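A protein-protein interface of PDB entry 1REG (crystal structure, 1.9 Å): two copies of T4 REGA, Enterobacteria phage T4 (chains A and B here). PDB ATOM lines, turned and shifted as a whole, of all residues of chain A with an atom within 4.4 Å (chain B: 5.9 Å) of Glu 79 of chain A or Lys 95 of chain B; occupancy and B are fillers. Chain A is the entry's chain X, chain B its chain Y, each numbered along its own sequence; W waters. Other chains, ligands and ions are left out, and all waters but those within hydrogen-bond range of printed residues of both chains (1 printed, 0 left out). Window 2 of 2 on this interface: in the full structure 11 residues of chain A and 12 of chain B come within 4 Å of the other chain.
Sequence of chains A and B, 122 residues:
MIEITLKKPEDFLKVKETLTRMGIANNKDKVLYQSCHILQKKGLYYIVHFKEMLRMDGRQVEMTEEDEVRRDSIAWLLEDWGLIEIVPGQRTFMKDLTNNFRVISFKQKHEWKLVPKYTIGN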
ATOM      1  N   ALA A  75       7.093  -8.174  17.389  1.00  0.00           N
ATOM      2  CA  ALA A  75       8.195  -7.784  16.535  1.00  0.00           C
ATOM      3  C   ALA A  75       8.599  -8.976  15.690  1.00  0.00           C
ATOM      4  O   ALA A  75       8.806  -8.779  14.509  1.00  0.00           O
ATOM      5  CB  ALA A  75       9.398  -7.330  17.337  1.00  0.00           C
ATOM      6  N   TRP A  76       8.714 -10.205  16.179  1.00  0.00           N
ATOM      7  CA  TRP A  76       8.957 -11.386  15.383  1.00  0.00           C
ATOM      8  C   TRP A  76       7.939 -11.613  14.304  1.00  0.00           C
ATOM      9  O   TRP A  76       8.381 -11.832  13.176  1.00  0.00           O
ATOM     10  CB  TRP A  76       9.001 -12.640  16.230  1.00  0.00           C
ATOM     11  CG  TRP A  76      10.325 -12.743  16.989  1.00  0.00           C
ATOM     12  CD1 TRP A  76      10.384 -12.795  18.373  1.00  0.00           C
ATOM     13  CD2 TRP A  76      11.554 -12.697  16.390  1.00  0.00           C
ATOM     14  NE1 TRP A  76      11.654 -12.750  18.630  1.00  0.00           N
ATOM     15  CE2 TRP A  76      12.379 -12.692  17.496  1.00  0.00           C
ATOM     16  CE3 TRP A  76      12.068 -12.657  15.112  1.00  0.00           C
ATOM     17  CZ2 TRP A  76      13.747 -12.636  17.331  1.00  0.00           C
ATOM     18  CZ3 TRP A  76      13.438 -12.607  14.956  1.00  0.00           C
ATOM     19  CH2 TRP A  76      14.274 -12.597  16.060  1.00  0.00           C
ATOM     20  N   LEU A  77       6.630 -11.532  14.582  1.00  0.00           N
ATOM     21  CA  LEU A  77       5.571 -11.659  13.604  1.00  0.00           C
ATOM     22  C   LEU A  77       5.686 -10.648  12.459  1.00  0.00           C
ATOM     23  O   LEU A  77       5.658 -11.033  11.295  1.00  0.00           O
ATOM     24  CB  LEU A  77       4.237 -11.523  14.334  1.00  0.00           C
ATOM     25  CG  LEU A  77       2.989 -12.004  13.546  1.00  0.00           C
ATOM     26  CD1 LEU A  77       3.217 -13.423  13.001  1.00  0.00           C
ATOM     27  CD2 LEU A  77       1.774 -11.943  14.433  1.00  0.00           C
ATOM     28  N   LEU A  78       5.841  -9.351  12.702  1.00  0.00           N
ATOM     29  CA  LEU A  78       6.078  -8.357  11.664  1.00  0.00           C
ATOM     30  C   LEU A  78       7.349  -8.717  10.900  1.00  0.00           C
ATOM     31  O   LEU A  78       7.359  -8.609   9.664  1.00  0.00           O
ATOM     32  CB  LEU A  78       6.192  -6.994  12.309  1.00  0.00           C
ATOM     33  CG  LEU A  78       4.885  -6.453  12.899  1.00  0.00           C
ATOM     34  CD1 LEU A  78       5.130  -5.216  13.695  1.00  0.00           C
ATOM     35  CD2 LEU A  78       3.933  -6.102  11.784  1.00  0.00           C
ATOM     36  N   GLU A  79       8.392  -9.214  11.564  1.00  0.00           N
ATOM     37  CA  GLU A  79       9.546  -9.696  10.841  1.00  0.00           C
ATOM     38  C   GLU A  79       9.213 -10.875   9.935  1.00  0.00           C
ATOM     39  O   GLU A  79       9.527 -10.785   8.752  1.00  0.00           O
ATOM     40  CB  GLU A  79      10.671 -10.104  11.784  1.00  0.00           C
ATOM     41  CG  GLU A  79      11.950 -10.173  10.957  1.00  0.00           C
ATOM     42  CD  GLU A  79      13.257 -10.454  11.688  1.00  0.00           C
ATOM     43  OE1 GLU A  79      13.433  -9.995  12.810  1.00  0.00           O
ATOM     44  OE2 GLU A  79      14.119 -11.138  11.141  1.00  0.00           O
ATOM     45  N   ASP A  80       8.522 -11.917  10.379  1.00  0.00           N
ATOM     46  CA  ASP A  80       8.137 -13.018   9.513  1.00  0.00           C
ATOM     47  C   ASP A  80       7.349 -12.587   8.292  1.00  0.00           C
ATOM     48  O   ASP A  80       7.544 -13.106   7.208  1.00  0.00           O
ATOM     49  CB  ASP A  80       7.292 -14.046  10.232  1.00  0.00           C
ATOM     50  CG  ASP A  80       8.044 -14.894  11.241  1.00  0.00           C
ATOM     51  OD1 ASP A  80       9.258 -15.082  11.170  1.00  0.00           O
ATOM     52  OD2 ASP A  80       7.408 -15.387  12.139  1.00  0.00           O
ATOM     53  N   TRP A  81       6.474 -11.595   8.443  1.00  0.00           N
ATOM     54  CA  TRP A  81       5.636 -11.113   7.364  1.00  0.00           C
ATOM     55  C   TRP A  81       6.409 -10.215   6.432  1.00  0.00           C
ATOM     56  O   TRP A  81       5.873  -9.721   5.458  1.00  0.00           O
ATOM     57  CB  TRP A  81       4.484 -10.309   7.899  1.00  0.00           C
ATOM     58  CG  TRP A  81       3.405 -11.067   8.645  1.00  0.00           C
ATOM     59  CD1 TRP A  81       3.209 -12.409   8.526  1.00  0.00           C
ATOM     60  CD2 TRP A  81       2.447 -10.465   9.411  1.00  0.00           C
ATOM     61  NE1 TRP A  81       2.128 -12.657   9.207  1.00  0.00           N
ATOM     62  CE2 TRP A  81       1.645 -11.533   9.752  1.00  0.00           C
ATOM     63  CE3 TRP A  81       2.141  -9.200   9.876  1.00  0.00           C
ATOM     64  CZ2 TRP A  81       0.520 -11.352  10.533  1.00  0.00           C
ATOM     65  CZ3 TRP A  81       1.010  -9.032  10.656  1.00  0.00           C
ATOM     66  CH2 TRP A  81       0.214 -10.100  10.991  1.00  0.00           C
ATOM     67  N   GLY A  82       7.655  -9.891   6.809  1.00  0.00           N
ATOM     68  CA  GLY A  82       8.517  -9.068   6.016  1.00  0.00           C
ATOM     69  C   GLY A  82       8.197  -7.592   6.114  1.00  0.00           C
ATOM     70  O   GLY A  82       8.650  -6.856   5.221  1.00  0.00           O
ATOM     71  N   ILE A  84       9.258  -5.682   8.731  1.00  0.00           N
ATOM     72  CA  ILE A  84      10.412  -5.099   9.436  1.00  0.00           C
ATOM     73  C   ILE A  84      11.497  -6.159   9.436  1.00  0.00           C
ATOM     74  O   ILE A  84      11.258  -7.297   9.030  1.00  0.00           O
ATOM     75  CB  ILE A  84      10.166  -4.728  10.964  1.00  0.00           C
ATOM     76  CG1 ILE A  84       9.803  -5.977  11.767  1.00  0.00           C
ATOM     77  CG2 ILE A  84       9.111  -3.646  11.064  1.00  0.00           C
ATOM     78  CD1 ILE A  84       9.385  -5.771  13.200  1.00  0.00           C
ATOM     79  N   GLU A  85      12.640  -5.768  10.010  1.00  0.00           N
ATOM     80  CA  GLU A  85      13.776  -6.634  10.280  1.00  0.00           C
ATOM     81  C   GLU A  85      14.168  -6.203  11.691  1.00  0.00           C
ATOM     82  O   GLU A  85      14.318  -4.995  11.914  1.00  0.00           O
ATOM     83  CB  GLU A  85      14.965  -6.327   9.388  1.00  0.00           C
ATOM     84  CG  GLU A  85      15.359  -7.143   8.131  1.00  0.00           C
ATOM     85  CD  GLU A  85      16.876  -7.009   7.891  1.00  0.00           C
ATOM     86  OE1 GLU A  85      17.681  -7.268   8.799  1.00  0.00           O
ATOM     87  OE2 GLU A  85      17.279  -6.597   6.802  1.00  0.00           O
ATOM     88  N   ILE A  86      14.263  -7.066  12.700  1.00  0.00           N
ATOM     89  CA  ILE A  86      14.768  -6.620  14.002  1.00  0.00           C
ATOM     90  C   ILE A  86      16.289  -6.417  13.904  1.00  0.00           C
ATOM     91  O   ILE A  86      16.970  -7.175  13.205  1.00  0.00           O
ATOM     92  CB  ILE A  86      14.362  -7.687  15.034  1.00  0.00           C
ATOM     93  CG1 ILE A  86      12.859  -7.803  15.052  1.00  0.00           C
ATOM     94  CG2 ILE A  86      14.798  -7.303  16.434  1.00  0.00           C
ATOM     95  CD1 ILE A  86      12.454  -8.954  15.977  1.00  0.00           C
ATOM     96  N   PRO A  88      20.099  -6.755  14.560  1.00  0.00           N
ATOM     97  CA  PRO A  88      20.996  -7.710  15.184  1.00  0.00           C
ATOM     98  C   PRO A  88      21.749  -7.129  16.353  1.00  0.00           C
ATOM     99  O   PRO A  88      22.096  -5.958  16.290  1.00  0.00           O
ATOM    100  CB  PRO A  88      21.881  -8.158  14.064  1.00  0.00           C
ATOM    101  CG  PRO A  88      21.719  -7.160  12.950  1.00  0.00           C
ATOM    102  CD  PRO A  88      20.299  -6.752  13.119  1.00  0.00           C
ATOM    103  N   GLY A  89      22.056  -7.911  17.388  1.00  0.00           N
ATOM    104  CA  GLY A  89      22.741  -7.413  18.582  1.00  0.00           C
ATOM    105  C   GLY A  89      21.758  -6.983  19.695  1.00  0.00           C
ATOM    106  O   GLY A  89      22.116  -6.216  20.602  1.00  0.00           O
ATOM    107  N   VAL B  69      26.808 -12.118  23.671  1.00  0.00           N
ATOM    108  CA  VAL B  69      26.444 -12.275  22.262  1.00  0.00           C
ATOM    109  C   VAL B  69      27.136 -13.564  21.805  1.00  0.00           C
ATOM    110  O   VAL B  69      26.436 -14.486  21.383  1.00  0.00           O
ATOM    111  CB  VAL B  69      26.939 -11.083  21.352  1.00  0.00           C
ATOM    112  CG1 VAL B  69      26.759 -11.430  19.857  1.00  0.00           C
ATOM    113  CG2 VAL B  69      26.137  -9.822  21.677  1.00  0.00           C
ATOM    114  N   SER B  73      25.147 -16.816  20.359  1.00  0.00           N
ATOM    115  CA  SER B  73      25.246 -17.204  18.961  1.00  0.00           C
ATOM    116  C   SER B  73      25.871 -18.576  18.858  1.00  0.00           C
ATOM    117  O   SER B  73      25.419 -19.316  18.001  1.00  0.00           O
ATOM    118  CB  SER B  73      26.064 -16.175  18.232  1.00  0.00           C
ATOM    119  OG  SER B  73      25.604 -14.880  18.607  1.00  0.00           O
ATOM    120  N   THR B  92      17.414 -13.966  24.689  1.00  0.00           N
ATOM    121  CA  THR B  92      18.787 -14.091  24.246  1.00  0.00           C
ATOM    122  C   THR B  92      19.068 -13.239  23.004  1.00  0.00           C
ATOM    123  O   THR B  92      18.184 -12.637  22.402  1.00  0.00           O
ATOM    124  CB  THR B  92      19.080 -15.631  24.014  1.00  0.00           C
ATOM    125  OG1 THR B  92      18.440 -16.002  22.804  1.00  0.00           O
ATOM    126  CG2 THR B  92      18.534 -16.573  25.092  1.00  0.00           C
ATOM    127  N   PHE B  93      20.336 -13.073  22.649  1.00  0.00           N
ATOM    128  CA  PHE B  93      20.689 -12.385  21.416  1.00  0.00           C
ATOM    129  C   PHE B  93      20.420 -13.473  20.385  1.00  0.00           C
ATOM    130  O   PHE B  93      21.020 -14.531  20.511  1.00  0.00           O
ATOM    131  CB  PHE B  93      22.178 -11.984  21.429  1.00  0.00           C
ATOM    132  CG  PHE B  93      22.567 -10.875  22.429  1.00  0.00           C
ATOM    133  CD1 PHE B  93      22.433  -9.535  22.068  1.00  0.00           C
ATOM    134  CD2 PHE B  93      23.090 -11.178  23.692  1.00  0.00           C
ATOM    135  CE1 PHE B  93      22.811  -8.527  22.944  1.00  0.00           C
ATOM    136  CE2 PHE B  93      23.468 -10.142  24.558  1.00  0.00           C
ATOM    137  CZ  PHE B  93      23.325  -8.818  24.186  1.00  0.00           C
ATOM    138  N   MET B  94      19.423 -13.341  19.536  1.00  0.00           N
ATOM    139  CA  MET B  94      19.051 -14.305  18.516  1.00  0.00           C
ATOM    140  C   MET B  94      19.554 -13.821  17.173  1.00  0.00           C
ATOM    141  O   MET B  94      19.412 -14.540  16.176  1.00  0.00           O
ATOM    142  CB  MET B  94      17.516 -14.457  18.457  1.00  0.00           C
ATOM    143  CG  MET B  94      16.923 -14.751  19.818  1.00  0.00           C
ATOM    144  SD  MET B  94      15.114 -14.656  19.883  1.00  0.00           S
ATOM    145  CE  MET B  94      14.627 -15.889  18.737  1.00  0.00           C
ATOM    146  N   LYS B  95      20.021 -12.580  16.980  1.00  0.00           N
ATOM    147  CA  LYS B  95      20.610 -12.141  15.726  1.00  0.00           C
ATOM    148  C   LYS B  95      21.986 -11.627  16.136  1.00  0.00           C
ATOM    149  O   LYS B  95      22.074 -10.714  16.964  1.00  0.00           O
ATOM    150  CB  LYS B  95      19.756 -11.021  15.088  1.00  0.00           C
ATOM    151  CG  LYS B  95      18.238 -11.393  15.087  1.00  0.00           C
ATOM    152  CD  LYS B  95      17.229 -10.452  14.443  1.00  0.00           C
ATOM    153  CE  LYS B  95      17.230 -10.686  12.935  1.00  0.00           C
ATOM    154  NZ  LYS B  95      16.586  -9.594  12.249  1.00  0.00           N
ATOM    155  N   ASP B  96      23.120 -12.140  15.643  1.00  0.00           N
ATOM    156  CA  ASP B  96      24.403 -11.576  16.096  1.00  0.00           C
ATOM    157  C   ASP B  96      24.696 -10.267  15.339  1.00  0.00           C
ATOM    158  O   ASP B  96      24.220 -10.007  14.223  1.00  0.00           O
ATOM    159  CB  ASP B  96      25.534 -12.615  15.863  1.00  0.00           C
ATOM    160  CG  ASP B  96      26.996 -12.291  16.258  1.00  0.00           C
ATOM    161  OD1 ASP B  96      27.587 -11.321  15.733  1.00  0.00           O
ATOM    162  OD2 ASP B  96      27.582 -13.050  17.061  1.00  0.00           O
ATOM    163  N   LEU B  97      25.553  -9.515  16.030  1.00  0.00           N
ATOM    164  CA  LEU B  97      26.311  -8.296  15.680  1.00  0.00           C
ATOM    165  C   LEU B  97      26.981  -8.160  17.052  1.00  0.00           C
ATOM    166  O   LEU B  97      26.348  -8.397  18.100  1.00  0.00           O
ATOM    167  CB  LEU B  97      25.497  -6.990  15.410  1.00  0.00           C
ATOM    168  CG  LEU B  97      26.087  -6.200  14.175  1.00  0.00           C
ATOM    169  CD1 LEU B  97      24.961  -5.853  13.181  1.00  0.00           C
ATOM    170  CD2 LEU B  97      26.808  -4.930  14.630  1.00  0.00           C
HETATM  171  O   HOH W   1      19.321  -8.828  17.524  1.00  0.00           O
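Printed residues of chain B that touch a printed residue of chain A: Phe 93, Met 94, Lys 95, Asp 96 and Leu 97.
Hydrophobic or aromatic side chains of chain B that line the printed part of chain A: Phe 93, Met 94 and Leu 97.
Of the 13 printed residues of chain A, 5 touch a printed residue of chain B.
Printed residues of chain A that touch a printed residue of chain B: Trp 76, Glu 79, Ile 86, Pro 88 and Gly 89.
Among the printed residues, 10 pairs touch across the chains.
Among the printed residues, Asp or Glu carboxylates within 4 Å of a Lys or Arg side-chain nitrogen of the other chain: Glu 79 of chain A with Lys 95 of chain B (3.1 Å).
Water W1 lies within hydrogen-bond range of N of Gly 89 of chain A (2.9 Å) and O of Lys 95 of chain B (3.4 Å).
The backbone carbonyl oxygen of Ile 86 of chain A is in hydrogen-bond range of the side-chain amino group of Lys 95 of chain B, 2.6 Å away.
The side-chain amino group (NZ) of Lys 95 of chain B lies within salt-bridge range of the side-chain carboxylate (OE2) of Glu 79 of chain A (3.1 Å).
The backbone NH (N) of Gly 89 of chain A sits at hydrogen-bond distance from the backbone carbonyl oxygen (O) of Lys 95 of chain B (2.8 Å).
SD of Met 94 of chain B touches CZ2 of Trp 76 of chain A (3.5 Å).
CD of Lys 95 of chain B touches CH2 of Trp 76 of chain A, 3.99 Å away.
Lys 95 of chain B touches Pro 88 of chain A.
Asp 96 of chain B touches Pro 88 of chain A.
Pro 88 of chain A touches Leu 97 of chain B.
O of Gly 89 of chain A touches CE1 of Phe 93 of chain B (3.4 Å).
CA of Gly 89 of chain A touches O of Leu 97 of chain B, 3.8 Å away.
No position is printed for both chains.
The side-chain hydroxyl (OG) of Ser 73 of chain B sits at hydrogen-bond distance from the side-chain carboxylate (OD2) of Asp 96 of chain B (3.1 Å).
The backbone NH of Ile 86 of chain A is in hydrogen-bond range of the side-chain carboxylate of Glu 79 of chain A (3.0 Å).
Of the printed residues of chain B, Trp 76 of chain A touches Met 94 (3.5 Å) and Lys 95 (3.99 Å).
Glu 79 of chain A touches just one residue of chain B: Lys 95.
Gly 82 of chain A touches none of the printed residues of chain B.
Of the printed residues of chain B, Ile 86 of chain A touches Lys 95 (2.6 Å).
Of the printed residues of chain B, Pro 88 of chain A touches Lys 95 (3.5 Å), Asp 96 (3.0 Å) and Leu 97 (3.5 Å).
Printed residues of chain B within 4 Å of Gly 89 of chain A: Phe 93, Lys 95 and Leu 97.
Val 69 of chain B touches none of the printed residues of chain A.
Printed residues of chain A within 4 Å of Lys 95 of chain B: Trp 76 (3.99 Å), Glu 79 (3.1 Å), Ile 86 (2.6 Å), Pro 88 (3.5 Å) and Gly 89 (2.8 Å).
Of the printed residues of chain A, Asp 96 of chain B touches Pro 88 (3.0 Å).
The nearest printed residue of chain A that does not touch Phe 93 of chain B is Pro 88 of chain A (6.2 Å).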
